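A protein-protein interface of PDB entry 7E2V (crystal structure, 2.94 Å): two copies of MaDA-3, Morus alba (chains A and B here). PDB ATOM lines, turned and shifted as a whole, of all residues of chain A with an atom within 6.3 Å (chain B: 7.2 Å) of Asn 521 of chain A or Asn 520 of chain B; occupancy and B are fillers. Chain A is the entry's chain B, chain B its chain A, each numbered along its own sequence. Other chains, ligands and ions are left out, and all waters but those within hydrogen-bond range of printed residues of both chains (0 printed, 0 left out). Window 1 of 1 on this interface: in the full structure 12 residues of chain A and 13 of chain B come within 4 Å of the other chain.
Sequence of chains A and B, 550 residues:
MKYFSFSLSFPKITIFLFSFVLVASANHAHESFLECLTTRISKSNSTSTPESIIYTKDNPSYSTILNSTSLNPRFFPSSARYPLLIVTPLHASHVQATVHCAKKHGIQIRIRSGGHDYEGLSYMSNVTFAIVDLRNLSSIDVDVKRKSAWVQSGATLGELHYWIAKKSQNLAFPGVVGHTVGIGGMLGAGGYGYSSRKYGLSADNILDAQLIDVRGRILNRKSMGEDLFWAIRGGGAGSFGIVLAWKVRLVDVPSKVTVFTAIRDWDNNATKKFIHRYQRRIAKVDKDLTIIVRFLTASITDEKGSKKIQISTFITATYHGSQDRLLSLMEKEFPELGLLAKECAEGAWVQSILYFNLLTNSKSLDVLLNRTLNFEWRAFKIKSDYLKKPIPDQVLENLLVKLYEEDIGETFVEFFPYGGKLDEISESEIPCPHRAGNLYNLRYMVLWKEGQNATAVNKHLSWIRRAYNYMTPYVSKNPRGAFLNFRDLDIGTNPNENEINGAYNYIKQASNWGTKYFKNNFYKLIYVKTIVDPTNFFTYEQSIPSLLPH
Among the printed residues, pairs that only touch across the chains: Trp 230 of chain A with Asn 520 of chain B (3.5 Å), Glu 427 of chain A with Ser 428 of chain B (3.9 Å), Ser 428 of chain A with Lys 519 of chain B (3.2 Å), Ser 428 of chain A with Asn 520 of chain B (3.4 Å), Lys 519 of chain A with Ser 428 of chain B (3.9 Å), Asn 520 of chain A with Trp 230 of chain B (3.6 Å), Asn 520 of chain A with Ser 428 of chain B (3.3 Å), Asn 520 of chain A with Lys 524 of chain B (3.8 Å), Tyr 523 of chain A with Lys 524 of chain B (3.5 Å), Lys 524 of chain A with Asn 520 of chain B (3.3 Å) and Lys 524 of chain A with Tyr 523 of chain B (3.6 Å).
ND2 of Asn 521 of chain B is in hydrogen-bond range of O of Glu 427 of chain B (2.8 Å).
The backbone carbonyl oxygen (O) of Ser 428 of chain B lies within hydrogen-bond range of the indole nitrogen (NE1) of Trp 230 of chain B (3.1 Å).
OD1 of Asn 521 of chain B is in hydrogen-bond range of ND2 of Asn 520 of chain A (3.2 Å).
The side-chain carboxylate (OE2) of Glu 427 of chain A lies within hydrogen-bond range of the backbone NH (N) of Glu 427 of chain B, at 3.4 Å.
OE1 of Glu 427 of chain B is in hydrogen-bond range of OG of Ser 428 of chain A (3.4 Å).
The side-chain amide nitrogen (ND2) of Asn 520 of chain B sits at hydrogen-bond distance from the side-chain amide oxygen (OD1) of Asn 521 of chain A (2.7 Å).
Of the printed residues of chain B, Trp 230 of chain A touches Asn 520.
Of the printed residues of chain B, Glu 427 of chain A touches Glu 427 (3.4 Å) and Ser 428 (3.9 Å).
Cys 432 of chain A touches none of the printed residues of chain B.
Of chain B, only Asn 520 comes within 4 Å of Asn 521 of chain A.
The nearest printed residue of chain B that does not touch Asn 521 of chain A is Glu 427 of chain B (6.4 Å).
The nearest residue of chain A that does not touch Asn 520 of chain B is Asn 520 of chain A (4.5 Å).
Of the 17 printed residues of chain B, 8 touch a printed residue of chain A.
Printed residues of chain B that touch a printed residue of chain A: Trp 230, Glu 427, Ser 428, Lys 519, Asn 520, Asn 521, Tyr 523 and Lys 524.
Hydrophobic or aromatic side chains of chain B that line the printed part of chain A: Trp 230 and Tyr 523.
Along chain B the printed residues that touch a printed residue of chain A span positions 230 to 524.
Hydrophobic or aromatic side chains of chain A within 4 Å of the printed part of chain B: Trp 230 and Tyr 523.
Glu 427 of chain A touches Ser 428 of chain B, and with the chains exchanged Ser 428 of chain A touches Glu 427 of chain B.
Asn 520 of chain A touches Asn 521 of chain B, and with the chains exchanged Asn 521 of chain A touches Asn 520 of chain B.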
ATOM      1  N   TRP A 230      23.432 -11.768   3.811  1.00  0.00           N
ATOM      2  CA  TRP A 230      23.544 -10.949   2.616  1.00  0.00           C
ATOM      3  C   TRP A 230      24.061  -9.565   2.970  1.00  0.00           C
ATOM      4  O   TRP A 230      24.931  -9.019   2.282  1.00  0.00           O
ATOM      5  CB  TRP A 230      22.179 -10.866   1.933  1.00  0.00           C
ATOM      6  CG  TRP A 230      22.113  -9.909   0.800  1.00  0.00           C
ATOM      7  CD1 TRP A 230      22.455 -10.150  -0.494  1.00  0.00           C
ATOM      8  CD2 TRP A 230      21.676  -8.543   0.854  1.00  0.00           C
ATOM      9  NE1 TRP A 230      22.258  -9.023  -1.254  1.00  0.00           N
ATOM     10  CE2 TRP A 230      21.781  -8.023  -0.450  1.00  0.00           C
ATOM     11  CE3 TRP A 230      21.207  -7.713   1.877  1.00  0.00           C
ATOM     12  CZ2 TRP A 230      21.435  -6.708  -0.760  1.00  0.00           C
ATOM     13  CZ3 TRP A 230      20.862  -6.406   1.565  1.00  0.00           C
ATOM     14  CH2 TRP A 230      20.981  -5.918   0.259  1.00  0.00           C
ATOM     15  N   GLU A 427      23.491  -7.501  -9.988  1.00  0.00           N
ATOM     16  CA  GLU A 427      23.571  -6.353  -9.090  1.00  0.00           C
ATOM     17  C   GLU A 427      23.029  -6.674  -7.701  1.00  0.00           C
ATOM     18  O   GLU A 427      23.407  -6.009  -6.729  1.00  0.00           O
ATOM     19  CB  GLU A 427      22.802  -5.171  -9.692  1.00  0.00           C
ATOM     20  CG  GLU A 427      23.093  -4.919 -11.168  1.00  0.00           C
ATOM     21  CD  GLU A 427      22.734  -3.512 -11.607  1.00  0.00           C
ATOM     22  OE1 GLU A 427      22.108  -2.776 -10.813  1.00  0.00           O
ATOM     23  OE2 GLU A 427      23.057  -3.143 -12.754  1.00  0.00           O
ATOM     24  N   SER A 428      22.160  -7.677  -7.585  1.00  0.00           N
ATOM     25  CA  SER A 428      21.564  -8.076  -6.316  1.00  0.00           C
ATOM     26  C   SER A 428      22.297  -9.228  -5.638  1.00  0.00           C
ATOM     27  O   SER A 428      21.861  -9.675  -4.574  1.00  0.00           O
ATOM     28  CB  SER A 428      20.096  -8.461  -6.525  1.00  0.00           C
ATOM     29  OG  SER A 428      19.982  -9.508  -7.473  1.00  0.00           O
ATOM     30  N   GLU A 429      23.394  -9.723  -6.220  1.00  0.00           N
ATOM     31  CA  GLU A 429      24.072 -10.881  -5.639  1.00  0.00           C
ATOM     32  C   GLU A 429      24.610 -10.558  -4.251  1.00  0.00           C
ATOM     33  O   GLU A 429      24.494 -11.370  -3.327  1.00  0.00           O
ATOM     34  CB  GLU A 429      25.201 -11.349  -6.560  1.00  0.00           C
ATOM     35  CG  GLU A 429      25.629 -12.801  -6.356  1.00  0.00           C
ATOM     36  CD  GLU A 429      24.462 -13.774  -6.399  1.00  0.00           C
ATOM     37  OE1 GLU A 429      23.687 -13.744  -7.380  1.00  0.00           O
ATOM     38  OE2 GLU A 429      24.321 -14.575  -5.453  1.00  0.00           O
ATOM     39  N   ILE A 430      25.198  -9.380  -4.089  1.00  0.00           N
ATOM     40  CA  ILE A 430      25.582  -8.839  -2.787  1.00  0.00           C
ATOM     41  C   ILE A 430      25.208  -7.361  -2.804  1.00  0.00           C
ATOM     42  O   ILE A 430      24.800  -6.850  -3.855  1.00  0.00           O
ATOM     43  CB  ILE A 430      27.078  -9.050  -2.497  1.00  0.00           C
ATOM     44  CG1 ILE A 430      27.923  -8.513  -3.647  1.00  0.00           C
ATOM     45  CG2 ILE A 430      27.383 -10.513  -2.216  1.00  0.00           C
ATOM     46  CD1 ILE A 430      29.390  -8.427  -3.332  1.00  0.00           C
ATOM     47  N   PRO A 431      25.302  -6.644  -1.680  1.00  0.00           N
ATOM     48  CA  PRO A 431      24.908  -5.227  -1.696  1.00  0.00           C
ATOM     49  C   PRO A 431      25.620  -4.389  -2.744  1.00  0.00           C
ATOM     50  O   PRO A 431      25.068  -3.366  -3.167  1.00  0.00           O
ATOM     51  CB  PRO A 431      25.253  -4.768  -0.277  1.00  0.00           C
ATOM     52  CG  PRO A 431      24.975  -5.962   0.544  1.00  0.00           C
ATOM     53  CD  PRO A 431      25.326  -7.167  -0.302  1.00  0.00           C
ATOM     54  N   CYS A 432      26.817  -4.776  -3.179  1.00  0.00           N
ATOM     55  CA  CYS A 432      27.511  -3.988  -4.197  1.00  0.00           C
ATOM     56  C   CYS A 432      26.791  -4.128  -5.532  1.00  0.00           C
ATOM     57  O   CYS A 432      26.689  -5.241  -6.064  1.00  0.00           O
ATOM     58  CB  CYS A 432      28.960  -4.432  -4.322  1.00  0.00           C
ATOM     59  SG  CYS A 432      29.928  -3.410  -5.452  1.00  0.00           S
ATOM     60  N   PRO A 433      26.278  -3.037  -6.110  1.00  0.00           N
ATOM     61  CA  PRO A 433      25.433  -3.118  -7.309  1.00  0.00           C
ATOM     62  C   PRO A 433      26.115  -2.841  -8.645  1.00  0.00           C
ATOM     63  O   PRO A 433      25.457  -2.979  -9.681  1.00  0.00           O
ATOM     64  CB  PRO A 433      24.405  -2.024  -7.018  1.00  0.00           C
ATOM     65  CG  PRO A 433      25.245  -0.960  -6.338  1.00  0.00           C
ATOM     66  CD  PRO A 433      26.369  -1.659  -5.606  1.00  0.00           C
ATOM     67  N   PHE A 518      24.767   1.696  -2.946  1.00  0.00           N
ATOM     68  CA  PHE A 518      23.997   0.497  -3.268  1.00  0.00           C
ATOM     69  C   PHE A 518      22.788   0.960  -4.065  1.00  0.00           C
ATOM     70  O   PHE A 518      21.894   1.606  -3.508  1.00  0.00           O
ATOM     71  CB  PHE A 518      23.543  -0.242  -2.006  1.00  0.00           C
ATOM     72  CG  PHE A 518      24.502  -0.141  -0.856  1.00  0.00           C
ATOM     73  CD1 PHE A 518      25.637  -0.932  -0.788  1.00  0.00           C
ATOM     74  CD2 PHE A 518      24.263   0.769   0.159  1.00  0.00           C
ATOM     75  CE1 PHE A 518      26.513  -0.817   0.284  1.00  0.00           C
ATOM     76  CE2 PHE A 518      25.130   0.890   1.226  1.00  0.00           C
ATOM     77  CZ  PHE A 518      26.255   0.098   1.291  1.00  0.00           C
ATOM     78  N   LYS A 519      22.739   0.614  -5.352  1.00  0.00           N
ATOM     79  CA  LYS A 519      21.778   1.217  -6.273  1.00  0.00           C
ATOM     80  C   LYS A 519      20.353   0.994  -5.786  1.00  0.00           C
ATOM     81  O   LYS A 519      19.658   1.954  -5.437  1.00  0.00           O
ATOM     82  CB  LYS A 519      21.961   0.655  -7.683  1.00  0.00           C
ATOM     83  CG  LYS A 519      23.265   1.075  -8.341  1.00  0.00           C
ATOM     84  CD  LYS A 519      23.268   0.826  -9.840  1.00  0.00           C
ATOM     85  CE  LYS A 519      24.193   1.810 -10.544  1.00  0.00           C
ATOM     86  NZ  LYS A 519      24.952   1.202 -11.675  1.00  0.00           N
ATOM     87  N   ASN A 520      19.900  -0.257  -5.766  1.00  0.00           N
ATOM     88  CA  ASN A 520      18.614  -0.581  -5.172  1.00  0.00           C
ATOM     89  C   ASN A 520      18.733  -1.520  -3.980  1.00  0.00           C
ATOM     90  O   ASN A 520      17.746  -1.710  -3.259  1.00  0.00           O
ATOM     91  CB  ASN A 520      17.665  -1.180  -6.222  1.00  0.00           C
ATOM     92  CG  ASN A 520      16.940  -0.110  -7.027  1.00  0.00           C
ATOM     93  OD1 ASN A 520      17.204   1.085  -6.872  1.00  0.00           O
ATOM     94  ND2 ASN A 520      16.008  -0.531  -7.876  1.00  0.00           N
ATOM     95  N   ASN A 521      19.915  -2.095  -3.745  1.00  0.00           N
ATOM     96  CA  ASN A 521      20.177  -2.880  -2.543  1.00  0.00           C
ATOM     97  C   ASN A 521      20.016  -2.060  -1.269  1.00  0.00           C
ATOM     98  O   ASN A 521      19.823  -2.635  -0.194  1.00  0.00           O
ATOM     99  CB  ASN A 521      21.576  -3.484  -2.631  1.00  0.00           C
ATOM    100  CG  ASN A 521      21.749  -4.354  -3.860  1.00  0.00           C
ATOM    101  OD1 ASN A 521      20.840  -5.095  -4.238  1.00  0.00           O
ATOM    102  ND2 ASN A 521      22.905  -4.254  -4.504  1.00  0.00           N
ATOM    103  N   PHE A 522      20.132  -0.732  -1.363  1.00  0.00           N
ATOM    104  CA  PHE A 522      19.944   0.140  -0.206  1.00  0.00           C
ATOM    105  C   PHE A 522      18.601  -0.108   0.472  1.00  0.00           C
ATOM    106  O   PHE A 522      18.503  -0.087   1.703  1.00  0.00           O
ATOM    107  CB  PHE A 522      20.077   1.596  -0.663  1.00  0.00           C
ATOM    108  CG  PHE A 522      19.477   2.621   0.276  1.00  0.00           C
ATOM    109  CD1 PHE A 522      20.191   3.070   1.374  1.00  0.00           C
ATOM    110  CD2 PHE A 522      18.243   3.196   0.009  1.00  0.00           C
ATOM    111  CE1 PHE A 522      19.668   4.036   2.215  1.00  0.00           C
ATOM    112  CE2 PHE A 522      17.716   4.165   0.849  1.00  0.00           C
ATOM    113  CZ  PHE A 522      18.436   4.586   1.951  1.00  0.00           C
ATOM    114  N   TYR A 523      17.555  -0.353  -0.318  1.00  0.00           N
ATOM    115  CA  TYR A 523      16.223  -0.578   0.239  1.00  0.00           C
ATOM    116  C   TYR A 523      16.141  -1.908   0.989  1.00  0.00           C
ATOM    117  O   TYR A 523      15.648  -1.963   2.128  1.00  0.00           O
ATOM    118  CB  TYR A 523      15.194  -0.479  -0.889  1.00  0.00           C
ATOM    119  CG  TYR A 523      15.214   0.899  -1.525  1.00  0.00           C
ATOM    120  CD1 TYR A 523      14.497   1.949  -0.966  1.00  0.00           C
ATOM    121  CD2 TYR A 523      15.988   1.161  -2.653  1.00  0.00           C
ATOM    122  CE1 TYR A 523      14.524   3.214  -1.524  1.00  0.00           C
ATOM    123  CE2 TYR A 523      16.022   2.424  -3.220  1.00  0.00           C
ATOM    124  CZ  TYR A 523      15.289   3.445  -2.651  1.00  0.00           C
ATOM    125  OH  TYR A 523      15.318   4.705  -3.205  1.00  0.00           O
ATOM    126  N   LYS A 524      16.619  -2.994   0.366  1.00  0.00           N
ATOM    127  CA  LYS A 524      16.744  -4.263   1.080  1.00  0.00           C
ATOM    128  C   LYS A 524      17.606  -4.083   2.322  1.00  0.00           C
ATOM    129  O   LYS A 524      17.346  -4.689   3.372  1.00  0.00           O
ATOM    130  CB  LYS A 524      17.339  -5.336   0.163  1.00  0.00           C
ATOM    131  CG  LYS A 524      17.196  -6.772   0.678  1.00  0.00           C
ATOM    132  CD  LYS A 524      18.036  -7.748  -0.149  1.00  0.00           C
ATOM    133  CE  LYS A 524      17.532  -9.185  -0.050  1.00  0.00           C
ATOM    134  NZ  LYS A 524      17.627  -9.730   1.334  1.00  0.00           N
ATOM    135  N   LEU A 525      18.656  -3.265   2.202  1.00  0.00           N
ATOM    136  CA  LEU A 525      19.512  -2.965   3.343  1.00  0.00           C
ATOM    137  C   LEU A 525      18.706  -2.376   4.492  1.00  0.00           C
ATOM    138  O   LEU A 525      18.847  -2.808   5.639  1.00  0.00           O
ATOM    139  CB  LEU A 525      20.633  -2.013   2.927  1.00  0.00           C
ATOM    140  CG  LEU A 525      21.918  -2.680   2.425  1.00  0.00           C
ATOM    141  CD1 LEU A 525      23.041  -1.672   2.301  1.00  0.00           C
ATOM    142  CD2 LEU A 525      22.330  -3.813   3.345  1.00  0.00           C
ATOM    143  N   ILE A 526      17.853  -1.384   4.206  1.00  0.00           N
ATOM    144  CA  ILE A 526      17.078  -0.767   5.282  1.00  0.00           C
ATOM    145  C   ILE A 526      16.130  -1.780   5.900  1.00  0.00           C
ATOM    146  O   ILE A 526      15.962  -1.825   7.122  1.00  0.00           O
ATOM    147  CB  ILE A 526      16.293   0.463   4.789  1.00  0.00           C
ATOM    148  CG1 ILE A 526      17.204   1.579   4.314  1.00  0.00           C
ATOM    149  CG2 ILE A 526      15.411   1.017   5.900  1.00  0.00           C
ATOM    150  CD1 ILE A 526      16.412   2.672   3.671  1.00  0.00           C
ATOM    151  N   TRP B 230       9.095   5.166 -11.806  1.00  0.00           N
ATOM    152  CA  TRP B 230       9.882   3.940 -11.916  1.00  0.00           C
ATOM    153  C   TRP B 230       9.030   2.712 -11.611  1.00  0.00           C
ATOM    154  O   TRP B 230       9.092   1.706 -12.330  1.00  0.00           O
ATOM    155  CB  TRP B 230      11.085   4.015 -10.973  1.00  0.00           C
ATOM    156  CG  TRP B 230      11.875   2.749 -10.875  1.00  0.00           C
ATOM    157  CD1 TRP B 230      12.908   2.372 -11.682  1.00  0.00           C
ATOM    158  CD2 TRP B 230      11.719   1.701  -9.906  1.00  0.00           C
ATOM    159  NE1 TRP B 230      13.393   1.156 -11.284  1.00  0.00           N
ATOM    160  CE2 TRP B 230      12.684   0.720 -10.197  1.00  0.00           C
ATOM    161  CE3 TRP B 230      10.856   1.496  -8.828  1.00  0.00           C
ATOM    162  CZ2 TRP B 230      12.813  -0.453  -9.452  1.00  0.00           C
ATOM    163  CZ3 TRP B 230      10.981   0.336  -8.087  1.00  0.00           C
ATOM    164  CH2 TRP B 230      11.954  -0.629  -8.401  1.00  0.00           C
ATOM    165  N   GLU B 427      19.837  -3.824 -13.608  1.00  0.00           N
ATOM    166  CA  GLU B 427      18.681  -4.453 -12.965  1.00  0.00           C
ATOM    167  C   GLU B 427      17.796  -3.446 -12.251  1.00  0.00           C
ATOM    168  O   GLU B 427      16.606  -3.705 -12.041  1.00  0.00           O
ATOM    169  CB  GLU B 427      19.076  -5.501 -11.922  1.00  0.00           C
ATOM    170  CG  GLU B 427      19.715  -6.762 -12.412  1.00  0.00           C
ATOM    171  CD  GLU B 427      19.875  -7.772 -11.283  1.00  0.00           C
ATOM    172  OE1 GLU B 427      19.610  -7.421 -10.112  1.00  0.00           O
ATOM    173  OE2 GLU B 427      20.215  -8.937 -11.571  1.00  0.00           O
ATOM    174  N   SER B 428      18.358  -2.314 -11.845  1.00  0.00           N
ATOM    175  CA  SER B 428      17.614  -1.310 -11.103  1.00  0.00           C
ATOM    176  C   SER B 428      17.053  -0.224 -12.001  1.00  0.00           C
ATOM    177  O   SER B 428      16.434   0.717 -11.500  1.00  0.00           O
ATOM    178  CB  SER B 428      18.511  -0.685 -10.035  1.00  0.00           C
ATOM    179  OG  SER B 428      19.374   0.280 -10.607  1.00  0.00           O
ATOM    180  N   PRO B 431      11.792  -1.861 -12.621  1.00  0.00           N
ATOM    181  CA  PRO B 431      11.624  -2.982 -11.681  1.00  0.00           C
ATOM    182  C   PRO B 431      12.043  -4.350 -12.194  1.00  0.00           C
ATOM    183  O   PRO B 431      12.379  -5.205 -11.366  1.00  0.00           O
ATOM    184  CB  PRO B 431      10.125  -2.937 -11.375  1.00  0.00           C
ATOM    185  CG  PRO B 431       9.825  -1.481 -11.398  1.00  0.00           C
ATOM    186  CD  PRO B 431      10.717  -0.868 -12.451  1.00  0.00           C
ATOM    187  N   PRO B 433      14.294  -7.198 -12.996  1.00  0.00           N
ATOM    188  CA  PRO B 433      15.699  -7.420 -12.600  1.00  0.00           C
ATOM    189  C   PRO B 433      16.476  -8.415 -13.453  1.00  0.00           C
ATOM    190  O   PRO B 433      17.651  -8.651 -13.156  1.00  0.00           O
ATOM    191  CB  PRO B 433      15.528  -7.976 -11.190  1.00  0.00           C
ATOM    192  CG  PRO B 433      14.303  -8.845 -11.333  1.00  0.00           C
ATOM    193  CD  PRO B 433      13.401  -8.182 -12.356  1.00  0.00           C
ATOM    194  N   PRO B 479      17.188 -15.797  -5.628  1.00  0.00           N
ATOM    195  CA  PRO B 479      15.871 -16.390  -5.884  1.00  0.00           C
ATOM    196  C   PRO B 479      15.781 -17.159  -7.197  1.00  0.00           C
ATOM    197  O   PRO B 479      16.653 -17.022  -8.051  1.00  0.00           O
ATOM    198  CB  PRO B 479      14.954 -15.171  -5.928  1.00  0.00           C
ATOM    199  CG  PRO B 479      15.829 -14.091  -6.462  1.00  0.00           C
ATOM    200  CD  PRO B 479      17.239 -14.383  -6.035  1.00  0.00           C
ATOM    201  N   GLY B 514       8.015 -11.980  -4.442  1.00  0.00           N
ATOM    202  CA  GLY B 514       8.587 -10.733  -4.924  1.00  0.00           C
ATOM    203  C   GLY B 514      10.003 -10.896  -5.444  1.00  0.00           C
ATOM    204  O   GLY B 514      10.323 -10.459  -6.551  1.00  0.00           O
ATOM    205  N   THR B 515      10.871 -11.531  -4.648  1.00  0.00           N
ATOM    206  CA  THR B 515      12.268 -11.691  -5.044  1.00  0.00           C
ATOM    207  C   THR B 515      12.402 -12.503  -6.324  1.00  0.00           C
ATOM    208  O   THR B 515      13.370 -12.321  -7.073  1.00  0.00           O
ATOM    209  CB  THR B 515      13.065 -12.348  -3.916  1.00  0.00           C
ATOM    210  OG1 THR B 515      12.371 -13.515  -3.454  1.00  0.00           O
ATOM    211  CG2 THR B 515      13.238 -11.385  -2.755  1.00  0.00           C
ATOM    212  N   TYR B 517       9.991 -12.479  -8.812  1.00  0.00           N
ATOM    213  CA  TYR B 517       9.618 -11.518  -9.849  1.00  0.00           C
ATOM    214  C   TYR B 517      10.617 -10.372  -9.930  1.00  0.00           C
ATOM    215  O   TYR B 517      11.092 -10.025 -11.019  1.00  0.00           O
ATOM    216  CB  TYR B 517       8.203 -10.989  -9.594  1.00  0.00           C
ATOM    217  CG  TYR B 517       7.087 -11.917 -10.032  1.00  0.00           C
ATOM    218  CD1 TYR B 517       7.314 -12.906 -10.970  1.00  0.00           C
ATOM    219  CD2 TYR B 517       5.812 -11.822  -9.491  1.00  0.00           C
ATOM    220  CE1 TYR B 517       6.300 -13.751 -11.392  1.00  0.00           C
ATOM    221  CE2 TYR B 517       4.796 -12.678  -9.898  1.00  0.00           C
ATOM    222  CZ  TYR B 517       5.046 -13.639 -10.848  1.00  0.00           C
ATOM    223  OH  TYR B 517       4.048 -14.498 -11.262  1.00  0.00           O
ATOM    224  N   PHE B 518      10.992  -9.813  -8.781  1.00  0.00           N
ATOM    225  CA  PHE B 518      11.819  -8.613  -8.697  1.00  0.00           C
ATOM    226  C   PHE B 518      12.940  -8.949  -7.727  1.00  0.00           C
ATOM    227  O   PHE B 518      12.694  -9.054  -6.521  1.00  0.00           O
ATOM    228  CB  PHE B 518      11.017  -7.419  -8.177  1.00  0.00           C
ATOM    229  CG  PHE B 518       9.599  -7.358  -8.682  1.00  0.00           C
ATOM    230  CD1 PHE B 518       9.287  -6.777  -9.902  1.00  0.00           C
ATOM    231  CD2 PHE B 518       8.576  -7.905  -7.931  1.00  0.00           C
ATOM    232  CE1 PHE B 518       7.973  -6.733 -10.345  1.00  0.00           C
ATOM    233  CE2 PHE B 518       7.270  -7.872  -8.364  1.00  0.00           C
ATOM    234  CZ  PHE B 518       6.965  -7.286  -9.574  1.00  0.00           C
ATOM    235  N   LYS B 519      14.171  -9.093  -8.229  1.00  0.00           N
ATOM    236  CA  LYS B 519      15.213  -9.705  -7.410  1.00  0.00           C
ATOM    237  C   LYS B 519      15.415  -8.921  -6.122  1.00  0.00           C
ATOM    238  O   LYS B 519      15.165  -9.451  -5.035  1.00  0.00           O
ATOM    239  CB  LYS B 519      16.525  -9.859  -8.185  1.00  0.00           C
ATOM    240  CG  LYS B 519      16.406 -10.915  -9.263  1.00  0.00           C
ATOM    241  CD  LYS B 519      17.658 -11.119 -10.089  1.00  0.00           C
ATOM    242  CE  LYS B 519      18.733 -11.846  -9.294  1.00  0.00           C
ATOM    243  NZ  LYS B 519      19.877 -12.207 -10.174  1.00  0.00           N
ATOM    244  N   ASN B 520      15.889  -7.681  -6.214  1.00  0.00           N
ATOM    245  CA  ASN B 520      15.927  -6.816  -5.046  1.00  0.00           C
ATOM    246  C   ASN B 520      15.095  -5.552  -5.209  1.00  0.00           C
ATOM    247  O   ASN B 520      14.748  -4.926  -4.196  1.00  0.00           O
ATOM    248  CB  ASN B 520      17.375  -6.430  -4.711  1.00  0.00           C
ATOM    249  CG  ASN B 520      18.045  -7.428  -3.786  1.00  0.00           C
ATOM    250  OD1 ASN B 520      17.420  -8.385  -3.325  1.00  0.00           O
ATOM    251  ND2 ASN B 520      19.324  -7.201  -3.502  1.00  0.00           N
ATOM    252  N   ASN B 521      14.688  -5.217  -6.440  1.00  0.00           N
ATOM    253  CA  ASN B 521      13.821  -4.064  -6.664  1.00  0.00           C
ATOM    254  C   ASN B 521      12.518  -4.195  -5.896  1.00  0.00           C
ATOM    255  O   ASN B 521      11.916  -3.180  -5.517  1.00  0.00           O
ATOM    256  CB  ASN B 521      13.535  -3.914  -8.160  1.00  0.00           C
ATOM    257  CG  ASN B 521      14.791  -3.964  -9.004  1.00  0.00           C
ATOM    258  OD1 ASN B 521      15.879  -3.622  -8.543  1.00  0.00           O
ATOM    259  ND2 ASN B 521      14.649  -4.429 -10.244  1.00  0.00           N
ATOM    260  N   PHE B 522      12.100  -5.434  -5.614  1.00  0.00           N
ATOM    261  CA  PHE B 522      10.877  -5.659  -4.855  1.00  0.00           C
ATOM    262  C   PHE B 522      10.904  -4.863  -3.564  1.00  0.00           C
ATOM    263  O   PHE B 522       9.916  -4.212  -3.205  1.00  0.00           O
ATOM    264  CB  PHE B 522      10.712  -7.152  -4.559  1.00  0.00           C
ATOM    265  CG  PHE B 522       9.789  -7.458  -3.403  1.00  0.00           C
ATOM    266  CD1 PHE B 522       8.419  -7.497  -3.590  1.00  0.00           C
ATOM    267  CD2 PHE B 522      10.293  -7.732  -2.140  1.00  0.00           C
ATOM    268  CE1 PHE B 522       7.565  -7.786  -2.540  1.00  0.00           C
ATOM    269  CE2 PHE B 522       9.442  -8.019  -1.084  1.00  0.00           C
ATOM    270  CZ  PHE B 522       8.076  -8.048  -1.288  1.00  0.00           C
ATOM    271  N   TYR B 523      12.066  -4.804  -2.915  1.00  0.00           N
ATOM    272  CA  TYR B 523      12.142  -4.064  -1.664  1.00  0.00           C
ATOM    273  C   TYR B 523      11.927  -2.578  -1.908  1.00  0.00           C
ATOM    274  O   TYR B 523      11.061  -1.959  -1.274  1.00  0.00           O
ATOM    275  CB  TYR B 523      13.472  -4.352  -0.972  1.00  0.00           C
ATOM    276  CG  TYR B 523      13.470  -5.734  -0.359  1.00  0.00           C
ATOM    277  CD1 TYR B 523      14.005  -6.821  -1.035  1.00  0.00           C
ATOM    278  CD2 TYR B 523      12.880  -5.959   0.878  1.00  0.00           C
ATOM    279  CE1 TYR B 523      13.981  -8.093  -0.480  1.00  0.00           C
ATOM    280  CE2 TYR B 523      12.850  -7.224   1.437  1.00  0.00           C
ATOM    281  CZ  TYR B 523      13.403  -8.287   0.758  1.00  0.00           C
ATOM    282  OH  TYR B 523      13.369  -9.545   1.323  1.00  0.00           O
ATOM    283  N   LYS B 524      12.630  -2.005  -2.890  1.00  0.00           N
ATOM    284  CA  LYS B 524      12.339  -0.620  -3.241  1.00  0.00           C
ATOM    285  C   LYS B 524      10.867  -0.468  -3.586  1.00  0.00           C
ATOM    286  O   LYS B 524      10.216   0.496  -3.162  1.00  0.00           O
ATOM    287  CB  LYS B 524      13.205  -0.146  -4.408  1.00  0.00           C
ATOM    288  CG  LYS B 524      12.620   1.094  -5.068  1.00  0.00           C
ATOM    289  CD  LYS B 524      13.610   1.894  -5.888  1.00  0.00           C
ATOM    290  CE  LYS B 524      12.899   3.089  -6.509  1.00  0.00           C
ATOM    291  NZ  LYS B 524      13.826   4.073  -7.126  1.00  0.00           N
ATOM    292  N   LEU B 525      10.307  -1.467  -4.280  1.00  0.00           N
ATOM    293  CA  LEU B 525       8.904  -1.414  -4.660  1.00  0.00           C
ATOM    294  C   LEU B 525       8.021  -1.199  -3.444  1.00  0.00           C
ATOM    295  O   LEU B 525       7.204  -0.268  -3.422  1.00  0.00           O
ATOM    296  CB  LEU B 525       8.513  -2.696  -5.404  1.00  0.00           C
ATOM    297  CG  LEU B 525       8.962  -2.782  -6.867  1.00  0.00           C
ATOM    298  CD1 LEU B 525       8.757  -4.170  -7.441  1.00  0.00           C
ATOM    299  CD2 LEU B 525       8.219  -1.767  -7.703  1.00  0.00           C
